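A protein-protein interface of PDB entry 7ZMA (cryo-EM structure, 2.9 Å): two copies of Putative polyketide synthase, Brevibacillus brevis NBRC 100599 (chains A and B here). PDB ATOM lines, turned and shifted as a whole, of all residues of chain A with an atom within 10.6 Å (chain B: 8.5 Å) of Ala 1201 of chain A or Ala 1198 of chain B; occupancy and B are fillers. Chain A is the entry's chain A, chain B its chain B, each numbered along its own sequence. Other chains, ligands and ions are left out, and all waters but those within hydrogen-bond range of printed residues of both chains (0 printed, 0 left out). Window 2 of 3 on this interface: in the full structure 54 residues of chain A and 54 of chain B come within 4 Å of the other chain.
Gln 1193 of chain A touches Leu 1194 of chain B (NE2 to CD1, 3.96 Å). Ser 1197 of chain B touches Leu 1194 of chain A (OG to CG, 2.9 Å). Ser 1197 of chain A touches Leu 1194 of chain B (OG to CG, 3.0 Å). Ser 1197 of chain A touches His 1268 of chain B. Ala 1198 of chain A touches Ala 1201 of chain B. Gln 1200 of chain A touches His 1268 of chain B. Ala 1198 of chain B touches Ala 1201 of chain A (CB to CB, 3.99 Å). Ser 1197 of chain B touches His 1268 of chain A. ND2 of Asn 1270 of chain A touches CB of Ala 1196 of chain B, at 3.996 Å. Gln 1200 of chain B touches Leu 1273 of chain A.
ND2 of Asn 1270 of chain A sits close to NE2 of Gln 1200 of chain B (3.3 Å).
OG of Ser 1197 of chain A sits at hydrogen-bond distance from O of Gln 1193 of chain A (3.4 Å). The backbone carbonyl oxygen (O) of Leu 1206 of chain A is in hydrogen-bond range of the side-chain amide nitrogen (NE2) of Gln 1200 of chain A, at 2.6 Å. ND1 of His 1268 of chain A sits close to N of Asn 1270 of chain A, 3.2 Å away. The backbone carbonyl oxygen (O) of Gln 1193 of chain B lies within hydrogen-bond range of the side-chain hydroxyl (OG) of Ser 1197 of chain B (3.4 Å). The side-chain amide nitrogen (NE2) of Gln 1200 of chain B sits at hydrogen-bond distance from the backbone carbonyl oxygen (O) of Leu 1206 of chain B (2.6 Å).
Printed residues of chain B within 4 Å of Gln 1193 of chain A: Leu 1194 (3.96 Å). Of the printed residues of chain B, Ala 1201 of chain A touches Ala 1198 (3.99 Å). Of the printed residues of chain B, Leu 1273 of chain A touches Gln 1200. Of the printed residues of chain A, Ala 1196 of chain B touches Asn 1270. Of the printed residues of chain A, Ala 1198 of chain B touches Ala 1201. No residue of chain A comes within 4 Å of Glu 1199 of chain B. Of the printed residues of chain A, Gln 1200 of chain B touches His 1268 (3.5 Å), Asn 1270 (3.3 Å) and Leu 1273 (3.8 Å). Of the printed residues of chain A, Ala 1201 of chain B touches Ala 1198 (3.9 Å). No residue of chain A comes within 4 Å of Leu 1202 of chain B. No residue of chain A comes within 4 Å of Gly 1203 of chain B. The nearest printed residue of chain B that does not touch Ala 1201 of chain A is Leu 1202 of chain B (4.4 Å). The nearest printed residue of chain A that does not touch Ala 1198 of chain B is Ser 1197 of chain A (4.7 Å). The nearest printed residue of chain B that does not touch Leu 1273 of chain A is Leu 1206 of chain B (4.7 Å).
Gln 1193 of chain A touches Leu 1194 of chain B, but with the chains exchanged Leu 1194 of chain A does not touch Gln 1193 of chain B (4.01 Å). Leu 1194 of chain A touches Ser 1197 of chain B, and with the chains exchanged Ser 1197 of chain A touches Leu 1194 of chain B. Ala 1198 of chain A touches Ala 1201 of chain B, and with the chains exchanged Ala 1201 of chain A touches Ala 1198 of chain B. Gln 1200 of chain A touches His 1268 of chain B, and with the chains exchanged His 1268 of chain A touches Gln 1200 of chain B. 16 positions are printed for both chains.
Of the 19 printed residues of chain A, 9 touch a printed residue of chain B. Printed residues of chain A that touch a printed residue of chain B: Gln 1193, Leu 1194, Ser 1197, Ala 1198, Gln 1200, Ala 1201, His 1268, Asn 1270 and Leu 1273. Hydrophobic or aromatic side chains of chain A that line the printed part of chain B: Leu 1194, Ala 1198, Ala 1201, His 1268 and Leu 1273. Of the 17 printed residues of chain B, 7 touch a printed residue of chain A. Along chain B the printed residues that touch a printed residue of chain A span positions 1194 to 1268. Among the printed residues, 12 pairs touch across the chains.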
ATOM      1  N   TYR A1106       3.267 -13.976  19.005  1.00  0.00           N
ATOM      2  CA  TYR A1106       4.325 -12.975  18.919  1.00  0.00           C
ATOM      3  C   TYR A1106       5.687 -13.432  18.410  1.00  0.00           C
ATOM      4  O   TYR A1106       6.529 -12.580  18.114  1.00  0.00           O
ATOM      5  CB  TYR A1106       4.453 -12.166  20.220  1.00  0.00           C
ATOM      6  CG  TYR A1106       3.258 -11.290  20.512  1.00  0.00           C
ATOM      7  CD1 TYR A1106       3.105 -10.059  19.890  1.00  0.00           C
ATOM      8  CD2 TYR A1106       2.283 -11.696  21.413  1.00  0.00           C
ATOM      9  CE1 TYR A1106       2.010  -9.257  20.156  1.00  0.00           C
ATOM     10  CE2 TYR A1106       1.187 -10.903  21.686  1.00  0.00           C
ATOM     11  CZ  TYR A1106       1.056  -9.684  21.055  1.00  0.00           C
ATOM     12  OH  TYR A1106      -0.035  -8.890  21.325  1.00  0.00           O
ATOM     13  N   GLN A1193      -3.531  -6.000  36.838  1.00  0.00           N
ATOM     14  CA  GLN A1193      -4.578  -5.066  36.443  1.00  0.00           C
ATOM     15  C   GLN A1193      -4.586  -4.789  34.946  1.00  0.00           C
ATOM     16  O   GLN A1193      -5.575  -4.250  34.431  1.00  0.00           O
ATOM     17  CB  GLN A1193      -4.410  -3.752  37.210  1.00  0.00           C
ATOM     18  CG  GLN A1193      -3.082  -3.058  36.966  1.00  0.00           C
ATOM     19  CD  GLN A1193      -2.902  -1.825  37.827  1.00  0.00           C
ATOM     20  OE1 GLN A1193      -3.789  -1.455  38.594  1.00  0.00           O
ATOM     21  NE2 GLN A1193      -1.745  -1.186  37.710  1.00  0.00           N
ATOM     22  N   LEU A1194      -3.511  -5.138  34.241  1.00  0.00           N
ATOM     23  CA  LEU A1194      -3.491  -5.015  32.791  1.00  0.00           C
ATOM     24  C   LEU A1194      -4.567  -5.872  32.138  1.00  0.00           C
ATOM     25  O   LEU A1194      -5.120  -5.478  31.104  1.00  0.00           O
ATOM     26  CB  LEU A1194      -2.101  -5.388  32.278  1.00  0.00           C
ATOM     27  CG  LEU A1194      -1.056  -4.272  32.402  1.00  0.00           C
ATOM     28  CD1 LEU A1194      -0.846  -3.877  33.848  1.00  0.00           C
ATOM     29  CD2 LEU A1194       0.270  -4.694  31.799  1.00  0.00           C
ATOM     30  N   TYR A1195      -4.898  -7.018  32.734  1.00  0.00           N
ATOM     31  CA  TYR A1195      -6.053  -7.785  32.285  1.00  0.00           C
ATOM     32  C   TYR A1195      -7.349  -7.012  32.477  1.00  0.00           C
ATOM     33  O   TYR A1195      -8.236  -7.076  31.620  1.00  0.00           O
ATOM     34  CB  TYR A1195      -6.125  -9.114  33.033  1.00  0.00           C
ATOM     35  CG  TYR A1195      -4.933 -10.003  32.790  1.00  0.00           C
ATOM     36  CD1 TYR A1195      -4.789 -10.684  31.591  1.00  0.00           C
ATOM     37  CD2 TYR A1195      -3.950 -10.154  33.753  1.00  0.00           C
ATOM     38  CE1 TYR A1195      -3.702 -11.495  31.360  1.00  0.00           C
ATOM     39  CE2 TYR A1195      -2.859 -10.963  33.532  1.00  0.00           C
ATOM     40  CZ  TYR A1195      -2.739 -11.630  32.334  1.00  0.00           C
ATOM     41  OH  TYR A1195      -1.653 -12.436  32.110  1.00  0.00           O
ATOM     42  N   ALA A1196      -7.478  -6.286  33.587  1.00  0.00           N
ATOM     43  CA  ALA A1196      -8.647  -5.438  33.784  1.00  0.00           C
ATOM     44  C   ALA A1196      -8.731  -4.378  32.696  1.00  0.00           C
ATOM     45  O   ALA A1196      -9.813  -4.088  32.176  1.00  0.00           O
ATOM     46  CB  ALA A1196      -8.595  -4.787  35.164  1.00  0.00           C
ATOM     47  N   SER A1197      -7.591  -3.778  32.347  1.00  0.00           N
ATOM     48  CA  SER A1197      -7.580  -2.780  31.281  1.00  0.00           C
ATOM     49  C   SER A1197      -7.990  -3.388  29.946  1.00  0.00           C
ATOM     50  O   SER A1197      -8.756  -2.783  29.186  1.00  0.00           O
ATOM     51  CB  SER A1197      -6.194  -2.154  31.173  1.00  0.00           C
ATOM     52  OG  SER A1197      -5.843  -1.517  32.384  1.00  0.00           O
ATOM     53  N   ALA A1198      -7.475  -4.579  29.635  1.00  0.00           N
ATOM     54  CA  ALA A1198      -7.860  -5.246  28.395  1.00  0.00           C
ATOM     55  C   ALA A1198      -9.354  -5.539  28.375  1.00  0.00           C
ATOM     56  O   ALA A1198     -10.024  -5.336  27.354  1.00  0.00           O
ATOM     57  CB  ALA A1198      -7.058  -6.535  28.223  1.00  0.00           C
ATOM     58  N   GLU A1199      -9.894  -6.019  29.497  1.00  0.00           N
ATOM     59  CA  GLU A1199     -11.327  -6.276  29.574  1.00  0.00           C
ATOM     60  C   GLU A1199     -12.120  -4.995  29.366  1.00  0.00           C
ATOM     61  O   GLU A1199     -13.116  -4.986  28.636  1.00  0.00           O
ATOM     62  CB  GLU A1199     -11.677  -6.907  30.922  1.00  0.00           C
ATOM     63  CG  GLU A1199     -11.245  -8.358  31.071  1.00  0.00           C
ATOM     64  CD  GLU A1199     -11.836  -9.260  30.006  1.00  0.00           C
ATOM     65  OE1 GLU A1199     -13.080  -9.345  29.920  1.00  0.00           O
ATOM     66  OE2 GLU A1199     -11.059  -9.884  29.253  1.00  0.00           O
ATOM     67  N   GLN A1200     -11.685  -3.898  29.990  1.00  0.00           N
ATOM     68  CA  GLN A1200     -12.378  -2.625  29.818  1.00  0.00           C
ATOM     69  C   GLN A1200     -12.366  -2.188  28.360  1.00  0.00           C
ATOM     70  O   GLN A1200     -13.388  -1.740  27.828  1.00  0.00           O
ATOM     71  CB  GLN A1200     -11.732  -1.553  30.695  1.00  0.00           C
ATOM     72  CG  GLN A1200     -12.048  -1.672  32.172  1.00  0.00           C
ATOM     73  CD  GLN A1200     -11.125  -0.831  33.029  1.00  0.00           C
ATOM     74  OE1 GLN A1200     -10.631   0.208  32.593  1.00  0.00           O
ATOM     75  NE2 GLN A1200     -10.884  -1.280  34.254  1.00  0.00           N
ATOM     76  N   ALA A1201     -11.214  -2.312  27.699  1.00  0.00           N
ATOM     77  CA  ALA A1201     -11.125  -1.920  26.297  1.00  0.00           C
ATOM     78  C   ALA A1201     -12.043  -2.772  25.430  1.00  0.00           C
ATOM     79  O   ALA A1201     -12.708  -2.257  24.522  1.00  0.00           O
ATOM     80  CB  ALA A1201      -9.681  -2.025  25.810  1.00  0.00           C
ATOM     81  N   LEU A1202     -12.093  -4.079  25.693  1.00  0.00           N
ATOM     82  CA  LEU A1202     -12.951  -4.952  24.899  1.00  0.00           C
ATOM     83  C   LEU A1202     -14.424  -4.764  25.240  1.00  0.00           C
ATOM     84  O   LEU A1202     -15.296  -5.160  24.458  1.00  0.00           O
ATOM     85  CB  LEU A1202     -12.545  -6.411  25.104  1.00  0.00           C
ATOM     86  CG  LEU A1202     -11.117  -6.768  24.689  1.00  0.00           C
ATOM     87  CD1 LEU A1202     -10.774  -8.183  25.126  1.00  0.00           C
ATOM     88  CD2 LEU A1202     -10.933  -6.611  23.186  1.00  0.00           C
ATOM     89  N   GLY A1203     -14.721  -4.168  26.393  1.00  0.00           N
ATOM     90  CA  GLY A1203     -16.091  -4.008  26.844  1.00  0.00           C
ATOM     91  C   GLY A1203     -16.232  -4.341  28.315  1.00  0.00           C
ATOM     92  O   GLY A1203     -15.316  -4.087  29.101  1.00  0.00           O
ATOM     93  N   ARG A1204     -17.374  -4.894  28.700  1.00  0.00           N
ATOM     94  CA  ARG A1204     -17.595  -5.385  30.062  1.00  0.00           C
ATOM     95  C   ARG A1204     -17.141  -4.313  31.057  1.00  0.00           C
ATOM     96  O   ARG A1204     -17.147  -3.116  30.749  1.00  0.00           O
ATOM     97  CB  ARG A1204     -16.905  -6.729  30.221  1.00  0.00           C
ATOM     98  CG  ARG A1204     -17.475  -7.832  29.347  1.00  0.00           C
ATOM     99  CD  ARG A1204     -16.867  -9.180  29.703  1.00  0.00           C
ATOM    100  NE  ARG A1204     -17.429 -10.268  28.911  1.00  0.00           N
ATOM    101  CZ  ARG A1204     -17.023 -11.529  28.977  1.00  0.00           C
ATOM    102  NH1 ARG A1204     -16.050 -11.901  29.792  1.00  0.00           N
ATOM    103  NH2 ARG A1204     -17.611 -12.441  28.207  1.00  0.00           N
ATOM    104  N   ALA A1205     -16.746  -4.729  32.260  1.00  0.00           N
ATOM    105  CA  ALA A1205     -16.192  -3.818  33.252  1.00  0.00           C
ATOM    106  C   ALA A1205     -15.547  -4.608  34.382  1.00  0.00           C
ATOM    107  O   ALA A1205     -16.163  -5.523  34.940  1.00  0.00           O
ATOM    108  CB  ALA A1205     -17.276  -2.889  33.799  1.00  0.00           C
ATOM    109  N   LEU A1206     -14.310  -4.264  34.727  1.00  0.00           N
ATOM    110  CA  LEU A1206     -13.577  -4.977  35.764  1.00  0.00           C
ATOM    111  C   LEU A1206     -12.492  -4.051  36.294  1.00  0.00           C
ATOM    112  O   LEU A1206     -11.874  -3.294  35.541  1.00  0.00           O
ATOM    113  CB  LEU A1206     -12.986  -6.283  35.223  1.00  0.00           C
ATOM    114  CG  LEU A1206     -12.010  -7.018  36.137  1.00  0.00           C
ATOM    115  CD1 LEU A1206     -12.694  -7.396  37.436  1.00  0.00           C
ATOM    116  CD2 LEU A1206     -11.452  -8.254  35.451  1.00  0.00           C
ATOM    117  N   ALA A1207     -12.266  -4.120  37.606  1.00  0.00           N
ATOM    118  CA  ALA A1207     -11.323  -3.216  38.251  1.00  0.00           C
ATOM    119  C   ALA A1207     -10.398  -3.927  39.231  1.00  0.00           C
ATOM    120  O   ALA A1207     -10.722  -4.051  40.416  1.00  0.00           O
ATOM    121  CB  ALA A1207     -12.078  -2.104  38.978  1.00  0.00           C
ATOM    122  N   HIS A1268       2.076 -11.626  32.129  1.00  0.00           N
ATOM    123  CA  HIS A1268       1.582 -10.836  31.009  1.00  0.00           C
ATOM    124  C   HIS A1268       2.680 -10.716  29.959  1.00  0.00           C
ATOM    125  O   HIS A1268       3.847 -10.471  30.311  1.00  0.00           O
ATOM    126  CB  HIS A1268       1.127  -9.447  31.485  1.00  0.00           C
ATOM    127  CG  HIS A1268       0.227  -8.739  30.520  1.00  0.00           C
ATOM    128  ND1 HIS A1268       0.523  -8.607  29.181  1.00  0.00           N
ATOM    129  CD2 HIS A1268      -0.972  -8.136  30.699  1.00  0.00           C
ATOM    130  CE1 HIS A1268      -0.450  -7.947  28.578  1.00  0.00           C
ATOM    131  NE2 HIS A1268      -1.370  -7.651  29.478  1.00  0.00           N
ATOM    132  N   ASN A1270       3.488  -8.385  28.082  1.00  0.00           N
ATOM    133  CA  ASN A1270       4.088  -7.059  27.987  1.00  0.00           C
ATOM    134  C   ASN A1270       5.518  -7.056  28.507  1.00  0.00           C
ATOM    135  O   ASN A1270       6.370  -6.326  27.988  1.00  0.00           O
ATOM    136  CB  ASN A1270       3.238  -6.047  28.758  1.00  0.00           C
ATOM    137  CG  ASN A1270       3.732  -4.621  28.604  1.00  0.00           C
ATOM    138  OD1 ASN A1270       4.928  -4.347  28.688  1.00  0.00           O
ATOM    139  ND2 ASN A1270       2.805  -3.701  28.377  1.00  0.00           N
ATOM    140  N   LEU A1273       7.598  -8.341  25.717  1.00  0.00           N
ATOM    141  CA  LEU A1273       7.542  -7.357  24.643  1.00  0.00           C
ATOM    142  C   LEU A1273       8.513  -6.214  24.908  1.00  0.00           C
ATOM    143  O   LEU A1273       9.275  -5.811  24.021  1.00  0.00           O
ATOM    144  CB  LEU A1273       6.113  -6.830  24.495  1.00  0.00           C
ATOM    145  CG  LEU A1273       5.250  -7.515  23.434  1.00  0.00           C
ATOM    146  CD1 LEU A1273       5.180  -9.008  23.681  1.00  0.00           C
ATOM    147  CD2 LEU A1273       3.858  -6.915  23.412  1.00  0.00           C
ATOM    148  N   TYR B1106     -19.221   6.269  31.635  1.00  0.00           N
ATOM    149  CA  TYR B1106     -19.399   5.528  32.877  1.00  0.00           C
ATOM    150  C   TYR B1106     -20.363   6.103  33.909  1.00  0.00           C
ATOM    151  O   TYR B1106     -20.706   5.398  34.862  1.00  0.00           O
ATOM    152  CB  TYR B1106     -18.052   5.154  33.517  1.00  0.00           C
ATOM    153  CG  TYR B1106     -17.251   4.161  32.709  1.00  0.00           C
ATOM    154  CD1 TYR B1106     -17.530   2.803  32.762  1.00  0.00           C
ATOM    155  CD2 TYR B1106     -16.211   4.585  31.892  1.00  0.00           C
ATOM    156  CE1 TYR B1106     -16.798   1.894  32.022  1.00  0.00           C
ATOM    157  CE2 TYR B1106     -15.474   3.686  31.148  1.00  0.00           C
ATOM    158  CZ  TYR B1106     -15.771   2.341  31.217  1.00  0.00           C
ATOM    159  OH  TYR B1106     -15.037   1.441  30.478  1.00  0.00           O
ATOM    160  N   TYR B1192      -0.030   4.116  33.355  1.00  0.00           N
ATOM    161  CA  TYR B1192       0.369   4.549  32.024  1.00  0.00           C
ATOM    162  C   TYR B1192       0.561   3.390  31.058  1.00  0.00           C
ATOM    163  O   TYR B1192       0.244   3.526  29.873  1.00  0.00           O
ATOM    164  CB  TYR B1192       1.669   5.357  32.115  1.00  0.00           C
ATOM    165  CG  TYR B1192       1.993   6.187  30.895  1.00  0.00           C
ATOM    166  CD1 TYR B1192       1.089   7.112  30.395  1.00  0.00           C
ATOM    167  CD2 TYR B1192       3.217   6.061  30.255  1.00  0.00           C
ATOM    168  CE1 TYR B1192       1.388   7.873  29.284  1.00  0.00           C
ATOM    169  CE2 TYR B1192       3.524   6.818  29.146  1.00  0.00           C
ATOM    170  CZ  TYR B1192       2.608   7.723  28.665  1.00  0.00           C
ATOM    171  OH  TYR B1192       2.915   8.480  27.559  1.00  0.00           O
ATOM    172  N   GLN B1193       1.070   2.255  31.540  1.00  0.00           N
ATOM    173  CA  GLN B1193       1.198   1.051  30.729  1.00  0.00           C
ATOM    174  C   GLN B1193      -0.141   0.378  30.457  1.00  0.00           C
ATOM    175  O   GLN B1193      -0.224  -0.475  29.564  1.00  0.00           O
ATOM    176  CB  GLN B1193       2.141   0.064  31.422  1.00  0.00           C
ATOM    177  CG  GLN B1193       1.673  -0.376  32.798  1.00  0.00           C
ATOM    178  CD  GLN B1193       2.682  -1.259  33.502  1.00  0.00           C
ATOM    179  OE1 GLN B1193       3.734  -1.583  32.950  1.00  0.00           O
ATOM    180  NE2 GLN B1193       2.371  -1.649  34.732  1.00  0.00           N
ATOM    181  N   LEU B1194      -1.184   0.738  31.205  1.00  0.00           N
ATOM    182  CA  LEU B1194      -2.517   0.229  30.927  1.00  0.00           C
ATOM    183  C   LEU B1194      -2.994   0.627  29.537  1.00  0.00           C
ATOM    184  O   LEU B1194      -3.720  -0.141  28.895  1.00  0.00           O
ATOM    185  CB  LEU B1194      -3.477   0.729  32.007  1.00  0.00           C
ATOM    186  CG  LEU B1194      -3.430  -0.065  33.318  1.00  0.00           C
ATOM    187  CD1 LEU B1194      -2.058   0.005  33.951  1.00  0.00           C
ATOM    188  CD2 LEU B1194      -4.465   0.443  34.303  1.00  0.00           C
ATOM    189  N   TYR B1195      -2.583   1.798  29.048  1.00  0.00           N
ATOM    190  CA  TYR B1195      -2.828   2.152  27.656  1.00  0.00           C
ATOM    191  C   TYR B1195      -2.113   1.208  26.702  1.00  0.00           C
ATOM    192  O   TYR B1195      -2.669   0.846  25.660  1.00  0.00           O
ATOM    193  CB  TYR B1195      -2.386   3.590  27.394  1.00  0.00           C
ATOM    194  CG  TYR B1195      -3.143   4.607  28.207  1.00  0.00           C
ATOM    195  CD1 TYR B1195      -4.447   4.948  27.882  1.00  0.00           C
ATOM    196  CD2 TYR B1195      -2.559   5.220  29.303  1.00  0.00           C
ATOM    197  CE1 TYR B1195      -5.145   5.873  28.622  1.00  0.00           C
ATOM    198  CE2 TYR B1195      -3.250   6.146  30.050  1.00  0.00           C
ATOM    199  CZ  TYR B1195      -4.543   6.468  29.704  1.00  0.00           C
ATOM    200  OH  TYR B1195      -5.234   7.390  30.447  1.00  0.00           O
ATOM    201  N   ALA B1196      -0.886   0.804  27.035  1.00  0.00           N
ATOM    202  CA  ALA B1196      -0.188  -0.183  26.221  1.00  0.00           C
ATOM    203  C   ALA B1196      -0.958  -1.494  26.187  1.00  0.00           C
ATOM    204  O   ALA B1196      -1.071  -2.135  25.137  1.00  0.00           O
ATOM    205  CB  ALA B1196       1.223  -0.405  26.763  1.00  0.00           C
ATOM    206  N   SER B1197      -1.489  -1.913  27.337  1.00  0.00           N
ATOM    207  CA  SER B1197      -2.280  -3.140  27.379  1.00  0.00           C
ATOM    208  C   SER B1197      -3.535  -3.022  26.525  1.00  0.00           C
ATOM    209  O   SER B1197      -3.897  -3.960  25.804  1.00  0.00           O
ATOM    210  CB  SER B1197      -2.650  -3.468  28.821  1.00  0.00           C
ATOM    211  OG  SER B1197      -1.487  -3.658  29.601  1.00  0.00           O
ATOM    212  N   ALA B1198      -4.223  -1.882  26.608  1.00  0.00           N
ATOM    213  CA  ALA B1198      -5.409  -1.678  25.782  1.00  0.00           C
ATOM    214  C   ALA B1198      -5.058  -1.721  24.301  1.00  0.00           C
ATOM    215  O   ALA B1198      -5.776  -2.332  23.498  1.00  0.00           O
ATOM    216  CB  ALA B1198      -6.071  -0.347  26.136  1.00  0.00           C
ATOM    217  N   GLU B1199      -3.953  -1.076  23.920  1.00  0.00           N
ATOM    218  CA  GLU B1199      -3.520  -1.114  22.528  1.00  0.00           C
ATOM    219  C   GLU B1199      -3.218  -2.539  22.093  1.00  0.00           C
ATOM    220  O   GLU B1199      -3.610  -2.956  21.000  1.00  0.00           O
ATOM    221  CB  GLU B1199      -2.291  -0.225  22.335  1.00  0.00           C
ATOM    222  CG  GLU B1199      -2.579   1.269  22.373  1.00  0.00           C
ATOM    223  CD  GLU B1199      -3.593   1.699  21.329  1.00  0.00           C
ATOM    224  OE1 GLU B1199      -3.330   1.494  20.126  1.00  0.00           O
ATOM    225  OE2 GLU B1199      -4.650   2.240  21.713  1.00  0.00           O
ATOM    226  N   GLN B1200      -2.533  -3.307  22.943  1.00  0.00           N
ATOM    227  CA  GLN B1200      -2.225  -4.693  22.606  1.00  0.00           C
ATOM    228  C   GLN B1200      -3.500  -5.500  22.407  1.00  0.00           C
ATOM    229  O   GLN B1200      -3.609  -6.282  21.455  1.00  0.00           O
ATOM    230  CB  GLN B1200      -1.370  -5.323  23.706  1.00  0.00           C
ATOM    231  CG  GLN B1200       0.077  -4.872  23.713  1.00  0.00           C
ATOM    232  CD  GLN B1200       0.785  -5.232  25.002  1.00  0.00           C
ATOM    233  OE1 GLN B1200       0.452  -6.223  25.650  1.00  0.00           O
ATOM    234  NE2 GLN B1200       1.766  -4.425  25.383  1.00  0.00           N
ATOM    235  N   ALA B1201      -4.478  -5.325  23.298  1.00  0.00           N
ATOM    236  CA  ALA B1201      -5.731  -6.059  23.168  1.00  0.00           C
ATOM    237  C   ALA B1201      -6.453  -5.690  21.880  1.00  0.00           C
ATOM    238  O   ALA B1201      -7.002  -6.562  21.195  1.00  0.00           O
ATOM    239  CB  ALA B1201      -6.624  -5.791  24.378  1.00  0.00           C
ATOM    240  N   LEU B1202      -6.466  -4.401  21.534  1.00  0.00           N
ATOM    241  CA  LEU B1202      -7.143  -3.979  20.311  1.00  0.00           C
ATOM    242  C   LEU B1202      -6.357  -4.371  19.065  1.00  0.00           C
ATOM    243  O   LEU B1202      -6.920  -4.397  17.964  1.00  0.00           O
ATOM    244  CB  LEU B1202      -7.373  -2.469  20.336  1.00  0.00           C
ATOM    245  CG  LEU B1202      -8.249  -1.948  21.477  1.00  0.00           C
ATOM    246  CD1 LEU B1202      -8.233  -0.429  21.508  1.00  0.00           C
ATOM    247  CD2 LEU B1202      -9.671  -2.470  21.350  1.00  0.00           C
ATOM    248  N   GLY B1203      -5.070  -4.678  19.214  1.00  0.00           N
ATOM    249  CA  GLY B1203      -4.219  -4.989  18.083  1.00  0.00           C
ATOM    250  C   GLY B1203      -2.873  -4.303  18.193  1.00  0.00           C
ATOM    251  O   GLY B1203      -2.352  -4.134  19.298  1.00  0.00           O
ATOM    252  N   ARG B1204      -2.300  -3.917  17.061  1.00  0.00           N
ATOM    253  CA  ARG B1204      -1.065  -3.129  17.030  1.00  0.00           C
ATOM    254  C   ARG B1204      -0.043  -3.767  17.977  1.00  0.00           C
ATOM    255  O   ARG B1204      -0.079  -4.976  18.229  1.00  0.00           O
ATOM    256  CB  ARG B1204      -1.397  -1.680  17.340  1.00  0.00           C
ATOM    257  CG  ARG B1204      -2.279  -1.003  16.306  1.00  0.00           C
ATOM    258  CD  ARG B1204      -2.403   0.486  16.584  1.00  0.00           C
ATOM    259  NE  ARG B1204      -3.207   1.172  15.579  1.00  0.00           N
ATOM    260  CZ  ARG B1204      -3.526   2.458  15.626  1.00  0.00           C
ATOM    261  NH1 ARG B1204      -3.124   3.236  16.619  1.00  0.00           N
ATOM    262  NH2 ARG B1204      -4.265   2.980  14.651  1.00  0.00           N
ATOM    263  N   ALA B1205       0.879  -2.963  18.504  1.00  0.00           N
ATOM    264  CA  ALA B1205       1.836  -3.430  19.498  1.00  0.00           C
ATOM    265  C   ALA B1205       2.541  -2.242  20.141  1.00  0.00           C
ATOM    266  O   ALA B1205       3.048  -1.361  19.440  1.00  0.00           O
ATOM    267  CB  ALA B1205       2.855  -4.380  18.866  1.00  0.00           C
ATOM    268  N   LEU B1206       2.578  -2.211  21.469  1.00  0.00           N
ATOM    269  CA  LEU B1206       3.185  -1.105  22.193  1.00  0.00           C
ATOM    270  C   LEU B1206       3.559  -1.600  23.582  1.00  0.00           C
ATOM    271  O   LEU B1206       2.836  -2.388  24.197  1.00  0.00           O
ATOM    272  CB  LEU B1206       2.236   0.095  22.263  1.00  0.00           C
ATOM    273  CG  LEU B1206       2.654   1.243  23.180  1.00  0.00           C
ATOM    274  CD1 LEU B1206       3.987   1.809  22.734  1.00  0.00           C
ATOM    275  CD2 LEU B1206       1.593   2.330  23.206  1.00  0.00           C
ATOM    276  N   HIS B1268      -6.126   7.418  34.158  1.00  0.00           N
ATOM    277  CA  HIS B1268      -6.864   6.266  33.658  1.00  0.00           C
ATOM    278  C   HIS B1268      -8.138   6.095  34.477  1.00  0.00           C
ATOM    279  O   HIS B1268      -8.096   6.206  35.715  1.00  0.00           O
ATOM    280  CB  HIS B1268      -5.998   4.997  33.723  1.00  0.00           C
ATOM    281  CG  HIS B1268      -6.492   3.879  32.858  1.00  0.00           C
ATOM    282  ND1 HIS B1268      -7.802   3.450  32.866  1.00  0.00           N
ATOM    283  CD2 HIS B1268      -5.851   3.111  31.945  1.00  0.00           C
ATOM    284  CE1 HIS B1268      -7.945   2.462  32.002  1.00  0.00           C
ATOM    285  NE2 HIS B1268      -6.776   2.237  31.429  1.00  0.00           N
